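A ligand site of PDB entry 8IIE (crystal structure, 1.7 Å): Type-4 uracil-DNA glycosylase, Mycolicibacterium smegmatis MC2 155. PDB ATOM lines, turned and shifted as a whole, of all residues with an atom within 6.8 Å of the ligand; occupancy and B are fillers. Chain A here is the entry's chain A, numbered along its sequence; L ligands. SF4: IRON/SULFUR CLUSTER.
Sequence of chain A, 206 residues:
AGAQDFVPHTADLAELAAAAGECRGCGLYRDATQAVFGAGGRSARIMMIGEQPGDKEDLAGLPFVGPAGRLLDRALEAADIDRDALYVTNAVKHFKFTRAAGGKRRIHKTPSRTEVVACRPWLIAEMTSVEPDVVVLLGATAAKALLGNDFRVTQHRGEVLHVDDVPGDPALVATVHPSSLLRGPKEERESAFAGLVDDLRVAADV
The side-chain sulfur (SG) of Cys 23 lies close to the backbone NH (N) of Gly 25 (3.2 Å).
The side-chain sulfur (SG) of Cys 23 sits close to the indole nitrogen (NE1) of Trp 122, 3.4 Å away.
SG of Cys 119 sits close to N of Lys 93 (3.5 Å).
O of Ala 91 lies close to SG of Cys 119, at 3.7 Å.
The backbone NH (N) of Leu 28 sits close to the side-chain sulfur (SG) of Cys 26 (3.6 Å).
A ring nitrogen (NE2) of His 94 lies within hydrogen-bond range of the backbone NH (N) of Ala 35 (3.2 Å).
O of Ala 118 sits at hydrogen-bond distance from N of Ala 3, 2.8 Å away.
An iron atom (FE3) of the ligand is bound by the side-chain sulfur of Cys 23, at 2.3 Å.
SG of Cys 119 is bound to FE1 of the ligand (2.3 Å).
N of Cys 26 sits close to S1 of the ligand (3.6 Å).
The side-chain sulfur (SG) of Cys 26 is bound to an iron atom (FE2) of the ligand, at 2.3 Å.
S3 of the ligand sits close to N of His 94 (3.7 Å).
An iron atom (FE4) of the ligand is bound by a ring nitrogen (ND1) of His 94 (2.4 Å).
The backbone NH of Gly 25 sits close to a sulfur (S1) of the ligand (3.7 Å).
NE1 of Trp 122 sits close to S2 of the ligand, at 3.7 Å.
Ala 3 touches the ligand (CB to S4, 3.9 Å).
Tyr 29 touches the ligand.
CB of Lys 93 touches S2 of the ligand, 3.6 Å away.
Ala 118 touches the ligand (O to S4, 3.9 Å).
Hydrophobic or aromatic side chains that line the ligand: Ala 3, Tyr 29, His 94 and Trp 122.
Of the 27 residues printed, 10 come within 4 Å of the ligand.
Along chain A the residues within 4 Å of the ligand span positions 3 to 122.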
ATOM      1  N   GLY A   2      11.504 -35.898   7.680  1.00  0.00           N
ATOM      2  CA  GLY A   2      10.395 -34.947   7.848  1.00  0.00           C
ATOM      3  C   GLY A   2      10.588 -34.012   9.045  1.00  0.00           C
ATOM      4  O   GLY A   2      11.645 -33.411   9.237  1.00  0.00           O
ATOM      5  N   ALA A   3       9.532 -33.871   9.859  1.00  0.00           N
ATOM      6  CA  ALA A   3       9.556 -32.912  10.990  1.00  0.00           C
ATOM      7  C   ALA A   3      10.362 -33.406  12.190  1.00  0.00           C
ATOM      8  O   ALA A   3      10.527 -32.647  13.115  1.00  0.00           O
ATOM      9  CB  ALA A   3       8.130 -32.751  11.485  1.00  0.00           C
ATOM     10  N   PHE A   6      12.807 -31.303  14.087  1.00  0.00           N
ATOM     11  CA  PHE A   6      12.304 -30.045  14.587  1.00  0.00           C
ATOM     12  C   PHE A   6      11.479 -30.202  15.862  1.00  0.00           C
ATOM     13  O   PHE A   6      11.129 -29.185  16.469  1.00  0.00           O
ATOM     14  CB  PHE A   6      11.445 -29.386  13.497  1.00  0.00           C
ATOM     15  CG  PHE A   6      12.235 -29.031  12.268  1.00  0.00           C
ATOM     16  CD1 PHE A   6      12.973 -27.874  12.240  1.00  0.00           C
ATOM     17  CD2 PHE A   6      12.237 -29.879  11.185  1.00  0.00           C
ATOM     18  CE1 PHE A   6      13.751 -27.533  11.088  1.00  0.00           C
ATOM     19  CE2 PHE A   6      13.021 -29.568  10.040  1.00  0.00           C
ATOM     20  CZ  PHE A   6      13.772 -28.361  10.036  1.00  0.00           C
ATOM     21  N   ALA A  20       6.944 -25.798  16.446  1.00  0.00           N
ATOM     22  CA  ALA A  20       6.319 -26.027  15.142  1.00  0.00           C
ATOM     23  C   ALA A  20       6.361 -24.778  14.273  1.00  0.00           C
ATOM     24  O   ALA A  20       6.436 -24.897  13.055  1.00  0.00           O
ATOM     25  CB  ALA A  20       4.873 -26.540  15.330  1.00  0.00           C
ATOM     26  N   GLY A  21       6.312 -23.582  14.902  1.00  0.00           N
ATOM     27  CA  GLY A  21       6.426 -22.343  14.145  1.00  0.00           C
ATOM     28  C   GLY A  21       7.729 -22.268  13.352  1.00  0.00           C
ATOM     29  O   GLY A  21       7.792 -21.609  12.293  1.00  0.00           O
ATOM     30  N   GLU A  22       8.695 -23.013  13.771  1.00  0.00           N
ATOM     31  CA  GLU A  22      10.021 -23.051  13.145  1.00  0.00           C
ATOM     32  C   GLU A  22      10.226 -24.205  12.194  1.00  0.00           C
ATOM     33  O   GLU A  22      11.339 -24.364  11.659  1.00  0.00           O
ATOM     34  CB  GLU A  22      11.079 -23.105  14.247  1.00  0.00           C
ATOM     35  CG  GLU A  22      11.043 -21.848  15.061  1.00  0.00           C
ATOM     36  CD  GLU A  22      11.276 -20.660  14.194  1.00  0.00           C
ATOM     37  OE1 GLU A  22      12.148 -20.777  13.282  1.00  0.00           O
ATOM     38  OE2 GLU A  22      10.542 -19.660  14.362  1.00  0.00           O
ATOM     39  N   CYS A  23       9.246 -25.138  12.147  1.00  0.00           N
ATOM     40  CA  CYS A  23       9.417 -26.385  11.421  1.00  0.00           C
ATOM     41  C   CYS A  23       9.624 -26.123   9.927  1.00  0.00           C
ATOM     42  O   CYS A  23       8.941 -25.280   9.333  1.00  0.00           O
ATOM     43  CB  CYS A  23       8.177 -27.282  11.626  1.00  0.00           C
ATOM     44  SG  CYS A  23       8.357 -28.936  10.853  1.00  0.00           S
ATOM     45  N   ARG A  24      10.582 -26.855   9.308  1.00  0.00           N
ATOM     46  CA  ARG A  24      10.757 -26.899   7.870  1.00  0.00           C
ATOM     47  C   ARG A  24      10.689 -28.346   7.369  1.00  0.00           C
ATOM     48  O   ARG A  24      11.282 -28.662   6.335  1.00  0.00           O
ATOM     49  CB  ARG A  24      12.101 -26.237   7.477  1.00  0.00           C
ATOM     50  CG  ARG A  24      12.230 -24.784   8.013  1.00  0.00           C
ATOM     51  CD  ARG A  24      13.484 -24.046   7.407  1.00  0.00           C
ATOM     52  NE  ARG A  24      14.676 -24.904   7.565  1.00  0.00           N
ATOM     53  CZ  ARG A  24      15.381 -24.998   8.690  1.00  0.00           C
ATOM     54  NH1 ARG A  24      15.046 -24.333   9.804  1.00  0.00           N
ATOM     55  NH2 ARG A  24      16.463 -25.793   8.706  1.00  0.00           N
ATOM     56  N   GLY A  25       9.946 -29.215   8.077  1.00  0.00           N
ATOM     57  CA  GLY A  25       9.945 -30.665   7.800  1.00  0.00           C
ATOM     58  C   GLY A  25       9.402 -31.058   6.436  1.00  0.00           C
ATOM     59  O   GLY A  25       9.656 -32.176   5.962  1.00  0.00           O
ATOM     60  N   CYS A  26       8.709 -30.126   5.790  1.00  0.00           N
ATOM     61  CA  CYS A  26       8.224 -30.286   4.395  1.00  0.00           C
ATOM     62  C   CYS A  26       8.180 -28.869   3.791  1.00  0.00           C
ATOM     63  O   CYS A  26       8.661 -27.953   4.413  1.00  0.00           O
ATOM     64  CB  CYS A  26       6.929 -31.069   4.251  1.00  0.00           C
ATOM     65  SG  CYS A  26       5.412 -30.174   4.715  1.00  0.00           S
ATOM     66  N   GLY A  27       7.630 -28.714   2.608  1.00  0.00           N
ATOM     67  CA  GLY A  27       7.699 -27.381   1.999  1.00  0.00           C
ATOM     68  C   GLY A  27       6.534 -26.473   2.337  1.00  0.00           C
ATOM     69  O   GLY A  27       6.548 -25.321   1.940  1.00  0.00           O
ATOM     70  N   LEU A  28       5.554 -26.982   3.059  1.00  0.00           N
ATOM     71  CA  LEU A  28       4.309 -26.195   3.263  1.00  0.00           C
ATOM     72  C   LEU A  28       4.527 -24.933   4.118  1.00  0.00           C
ATOM     73  O   LEU A  28       3.694 -24.066   4.084  1.00  0.00           O
ATOM     74  CB  LEU A  28       3.252 -27.095   3.887  1.00  0.00           C
ATOM     75  CG  LEU A  28       2.772 -28.221   2.980  1.00  0.00           C
ATOM     76  CD1 LEU A  28       1.713 -29.078   3.655  1.00  0.00           C
ATOM     77  CD2 LEU A  28       2.287 -27.670   1.655  1.00  0.00           C
ATOM     78  N   TYR A  29       5.609 -24.921   4.889  1.00  0.00           N
ATOM     79  CA  TYR A  29       5.799 -23.773   5.800  1.00  0.00           C
ATOM     80  C   TYR A  29       6.033 -22.502   4.981  1.00  0.00           C
ATOM     81  O   TYR A  29       5.799 -21.406   5.458  1.00  0.00           O
ATOM     82  CB  TYR A  29       7.021 -23.970   6.702  1.00  0.00           C
ATOM     83  CG  TYR A  29       8.353 -23.872   6.004  1.00  0.00           C
ATOM     84  CD1 TYR A  29       8.870 -24.943   5.303  1.00  0.00           C
ATOM     85  CD2 TYR A  29       9.104 -22.712   6.053  1.00  0.00           C
ATOM     86  CE1 TYR A  29      10.085 -24.859   4.643  1.00  0.00           C
ATOM     87  CE2 TYR A  29      10.316 -22.607   5.401  1.00  0.00           C
ATOM     88  CZ  TYR A  29      10.810 -23.686   4.699  1.00  0.00           C
ATOM     89  OH  TYR A  29      11.999 -23.589   4.046  1.00  0.00           O
ATOM     90  N   ARG A  30       6.495 -22.685   3.749  1.00  0.00           N
ATOM     91  CA  ARG A  30       6.921 -21.505   2.947  1.00  0.00           C
ATOM     92  C   ARG A  30       5.784 -20.522   2.631  1.00  0.00           C
ATOM     93  O   ARG A  30       5.995 -19.353   2.833  1.00  0.00           O
ATOM     94  CB  ARG A  30       7.631 -21.960   1.674  1.00  0.00           C
ATOM     95  CG  ARG A  30       9.027 -22.502   1.919  1.00  0.00           C
ATOM     96  CD  ARG A  30       9.610 -23.192   0.696  1.00  0.00           C
ATOM     97  NE  ARG A  30       8.672 -24.117   0.080  1.00  0.00           N
ATOM     98  CZ  ARG A  30       9.024 -25.060  -0.779  1.00  0.00           C
ATOM     99  NH1 ARG A  30      10.301 -25.202  -1.095  1.00  0.00           N
ATOM    100  NH2 ARG A  30       8.121 -25.861  -1.298  1.00  0.00           N
ATOM    101  N   ALA A  35       2.381 -21.759  11.467  1.00  0.00           N
ATOM    102  CA  ALA A  35       1.931 -23.119  11.792  1.00  0.00           C
ATOM    103  C   ALA A  35       0.692 -22.994  12.677  1.00  0.00           C
ATOM    104  O   ALA A  35       0.635 -22.049  13.449  1.00  0.00           O
ATOM    105  CB  ALA A  35       3.013 -23.834  12.552  1.00  0.00           C
ATOM    106  N   ALA A  91      -3.679 -33.147  10.996  1.00  0.00           N
ATOM    107  CA  ALA A  91      -2.581 -34.035  10.535  1.00  0.00           C
ATOM    108  C   ALA A  91      -1.391 -33.214  10.010  1.00  0.00           C
ATOM    109  O   ALA A  91      -0.266 -33.625  10.257  1.00  0.00           O
ATOM    110  CB  ALA A  91      -3.103 -34.993   9.501  1.00  0.00           C
ATOM    111  N   VAL A  92      -1.684 -32.141   9.273  1.00  0.00           N
ATOM    112  CA  VAL A  92      -0.612 -31.212   8.805  1.00  0.00           C
ATOM    113  C   VAL A  92      -0.836 -29.834   9.438  1.00  0.00           C
ATOM    114  O   VAL A  92      -1.987 -29.465   9.587  1.00  0.00           O
ATOM    115  CB  VAL A  92      -0.392 -31.176   7.279  1.00  0.00           C
ATOM    116  CG1 VAL A  92      -0.441 -32.563   6.653  1.00  0.00           C
ATOM    117  CG2 VAL A  92      -1.232 -30.175   6.516  1.00  0.00           C
ATOM    118  N   LYS A  93       0.259 -29.156   9.793  1.00  0.00           N
ATOM    119  CA  LYS A  93       0.166 -27.893  10.585  1.00  0.00           C
ATOM    120  C   LYS A  93       0.294 -26.612   9.750  1.00  0.00           C
ATOM    121  O   LYS A  93       0.109 -25.567  10.297  1.00  0.00           O
ATOM    122  CB  LYS A  93       1.309 -27.843  11.595  1.00  0.00           C
ATOM    123  CG  LYS A  93       1.061 -28.389  12.986  1.00  0.00           C
ATOM    124  CD  LYS A  93       0.255 -29.646  13.057  1.00  0.00           C
ATOM    125  CE  LYS A  93       0.139 -30.175  14.463  1.00  0.00           C
ATOM    126  NZ  LYS A  93      -0.378 -31.560  14.462  1.00  0.00           N
ATOM    127  N   HIS A  94       0.640 -26.735   8.467  1.00  0.00           N
ATOM    128  CA  HIS A  94       0.742 -25.566   7.562  1.00  0.00           C
ATOM    129  C   HIS A  94      -0.285 -25.709   6.422  1.00  0.00           C
ATOM    130  O   HIS A  94      -0.373 -26.765   5.847  1.00  0.00           O
ATOM    131  CB  HIS A  94       2.180 -25.302   7.100  1.00  0.00           C
ATOM    132  CG  HIS A  94       3.099 -24.555   8.042  1.00  0.00           C
ATOM    133  ND1 HIS A  94       4.115 -25.166   8.751  1.00  0.00           N
ATOM    134  CD2 HIS A  94       3.237 -23.232   8.309  1.00  0.00           C
ATOM    135  CE1 HIS A  94       4.789 -24.257   9.438  1.00  0.00           C
ATOM    136  NE2 HIS A  94       4.293 -23.030   9.168  1.00  0.00           N
ATOM    137  N   PHE A  95      -1.053 -24.640   6.202  1.00  0.00           N
ATOM    138  CA  PHE A  95      -2.091 -24.613   5.161  1.00  0.00           C
ATOM    139  C   PHE A  95      -1.478 -24.783   3.771  1.00  0.00           C
ATOM    140  O   PHE A  95      -0.583 -24.027   3.445  1.00  0.00           O
ATOM    141  CB  PHE A  95      -2.784 -23.258   5.283  1.00  0.00           C
ATOM    142  CG  PHE A  95      -3.909 -22.922   4.350  1.00  0.00           C
ATOM    143  CD1 PHE A  95      -4.829 -23.867   3.921  1.00  0.00           C
ATOM    144  CD2 PHE A  95      -4.093 -21.609   3.934  1.00  0.00           C
ATOM    145  CE1 PHE A  95      -5.879 -23.523   3.099  1.00  0.00           C
ATOM    146  CE2 PHE A  95      -5.143 -21.264   3.113  1.00  0.00           C
ATOM    147  CZ  PHE A  95      -6.028 -22.223   2.682  1.00  0.00           C
ATOM    148  N   GLU A 115       3.692 -35.439   2.716  1.00  0.00           N
ATOM    149  CA  GLU A 115       3.589 -34.314   3.706  1.00  0.00           C
ATOM    150  C   GLU A 115       2.964 -34.813   5.014  1.00  0.00           C
ATOM    151  O   GLU A 115       3.364 -34.395   6.071  1.00  0.00           O
ATOM    152  CB  GLU A 115       2.792 -33.167   3.088  1.00  0.00           C
ATOM    153  CG  GLU A 115       3.542 -32.466   1.989  1.00  0.00           C
ATOM    154  CD  GLU A 115       2.690 -31.754   0.954  1.00  0.00           C
ATOM    155  OE1 GLU A 115       1.514 -32.075   0.842  1.00  0.00           O
ATOM    156  OE2 GLU A 115       3.237 -30.881   0.285  1.00  0.00           O
ATOM    157  N   VAL A 117       3.165 -37.805   6.306  1.00  0.00           N
ATOM    158  CA  VAL A 117       4.190 -38.596   7.056  1.00  0.00           C
ATOM    159  C   VAL A 117       5.256 -37.650   7.592  1.00  0.00           C
ATOM    160  O   VAL A 117       5.721 -37.861   8.698  1.00  0.00           O
ATOM    161  CB  VAL A 117       4.740 -39.753   6.187  1.00  0.00           C
ATOM    162  CG1 VAL A 117       6.002 -40.368   6.772  1.00  0.00           C
ATOM    163  CG2 VAL A 117       3.701 -40.813   5.949  1.00  0.00           C
ATOM    164  N   ALA A 118       5.583 -36.618   6.822  1.00  0.00           N
ATOM    165  CA  ALA A 118       6.565 -35.617   7.291  1.00  0.00           C
ATOM    166  C   ALA A 118       6.078 -34.963   8.585  1.00  0.00           C
ATOM    167  O   ALA A 118       6.894 -34.764   9.458  1.00  0.00           O
ATOM    168  CB  ALA A 118       6.783 -34.573   6.213  1.00  0.00           C
ATOM    169  N   CYS A 119       4.781 -34.653   8.659  1.00  0.00           N
ATOM    170  CA  CYS A 119       4.232 -33.862   9.796  1.00  0.00           C
ATOM    171  C   CYS A 119       3.840 -34.737  10.996  1.00  0.00           C
ATOM    172  O   CYS A 119       3.721 -34.219  12.079  1.00  0.00           O
ATOM    173  CB  CYS A 119       3.061 -33.030   9.282  1.00  0.00           C
ATOM    174  SG  CYS A 119       2.757 -31.548  10.285  1.00  0.00           S
ATOM    175  N   ARG A 120       3.645 -36.015  10.713  1.00  0.00           N
ATOM    176  CA  ARG A 120       3.204 -36.975  11.768  1.00  0.00           C
ATOM    177  C   ARG A 120       4.007 -36.847  13.071  1.00  0.00           C
ATOM    178  O   ARG A 120       3.386 -37.002  14.116  1.00  0.00           O
ATOM    179  CB  ARG A 120       3.115 -38.422  11.243  1.00  0.00           C
ATOM    180  CG  ARG A 120       2.230 -39.316  12.093  1.00  0.00           C
ATOM    181  CD  ARG A 120       1.923 -40.610  11.365  1.00  0.00           C
ATOM    182  NE  ARG A 120       3.131 -41.251  10.865  1.00  0.00           N
ATOM    183  CZ  ARG A 120       3.131 -42.200   9.933  1.00  0.00           C
ATOM    184  NH1 ARG A 120       1.992 -42.622   9.426  1.00  0.00           N
ATOM    185  NH2 ARG A 120       4.271 -42.736   9.543  1.00  0.00           N
ATOM    186  N   PRO A 121       5.330 -36.639  13.096  1.00  0.00           N
ATOM    187  CA  PRO A 121       6.019 -36.490  14.378  1.00  0.00           C
ATOM    188  C   PRO A 121       5.360 -35.485  15.354  1.00  0.00           C
ATOM    189  O   PRO A 121       5.399 -35.675  16.516  1.00  0.00           O
ATOM    190  CB  PRO A 121       7.421 -36.028  13.963  1.00  0.00           C
ATOM    191  CG  PRO A 121       7.667 -36.745  12.677  1.00  0.00           C
ATOM    192  CD  PRO A 121       6.312 -36.720  12.000  1.00  0.00           C
ATOM    193  N   TRP A 122       4.780 -34.420  14.790  1.00  0.00           N
ATOM    194  CA  TRP A 122       4.034 -33.453  15.652  1.00  0.00           C
ATOM    195  C   TRP A 122       2.815 -34.143  16.283  1.00  0.00           C
ATOM    196  O   TRP A 122       2.581 -33.940  17.445  1.00  0.00           O
ATOM    197  CB  TRP A 122       3.642 -32.179  14.891  1.00  0.00           C
ATOM    198  CG  TRP A 122       4.811 -31.347  14.502  1.00  0.00           C
ATOM    199  CD1 TRP A 122       5.246 -31.085  13.233  1.00  0.00           C
ATOM    200  CD2 TRP A 122       5.716 -30.653  15.384  1.00  0.00           C
ATOM    201  NE1 TRP A 122       6.368 -30.300  13.276  1.00  0.00           N
ATOM    202  CE2 TRP A 122       6.675 -30.016  14.576  1.00  0.00           C
ATOM    203  CE3 TRP A 122       5.806 -30.520  16.777  1.00  0.00           C
ATOM    204  CZ2 TRP A 122       7.711 -29.258  15.119  1.00  0.00           C
ATOM    205  CZ3 TRP A 122       6.816 -29.771  17.306  1.00  0.00           C
ATOM    206  CH2 TRP A 122       7.755 -29.152  16.489  1.00  0.00           C
HETATM  207 FE1  SF4 L   1       4.186 -30.050   9.275  1.00  0.00          FE
HETATM  208 FE2  SF4 L   1       5.540 -29.546   6.958  1.00  0.00          FE
HETATM  209 FE3  SF4 L   1       6.620 -28.961   9.394  1.00  0.00          FE
HETATM  210 FE4  SF4 L   1       4.592 -27.518   8.437  1.00  0.00          FE
HETATM  211  S1  SF4 L   1       6.702 -27.623   7.492  1.00  0.00           S
HETATM  212  S2  SF4 L   1       4.766 -28.293  10.587  1.00  0.00           S
HETATM  213  S3  SF4 L   1       3.311 -29.059   7.379  1.00  0.00           S
HETATM  214  S4  SF4 L   1       6.146 -31.041   8.556  1.00  0.00           S
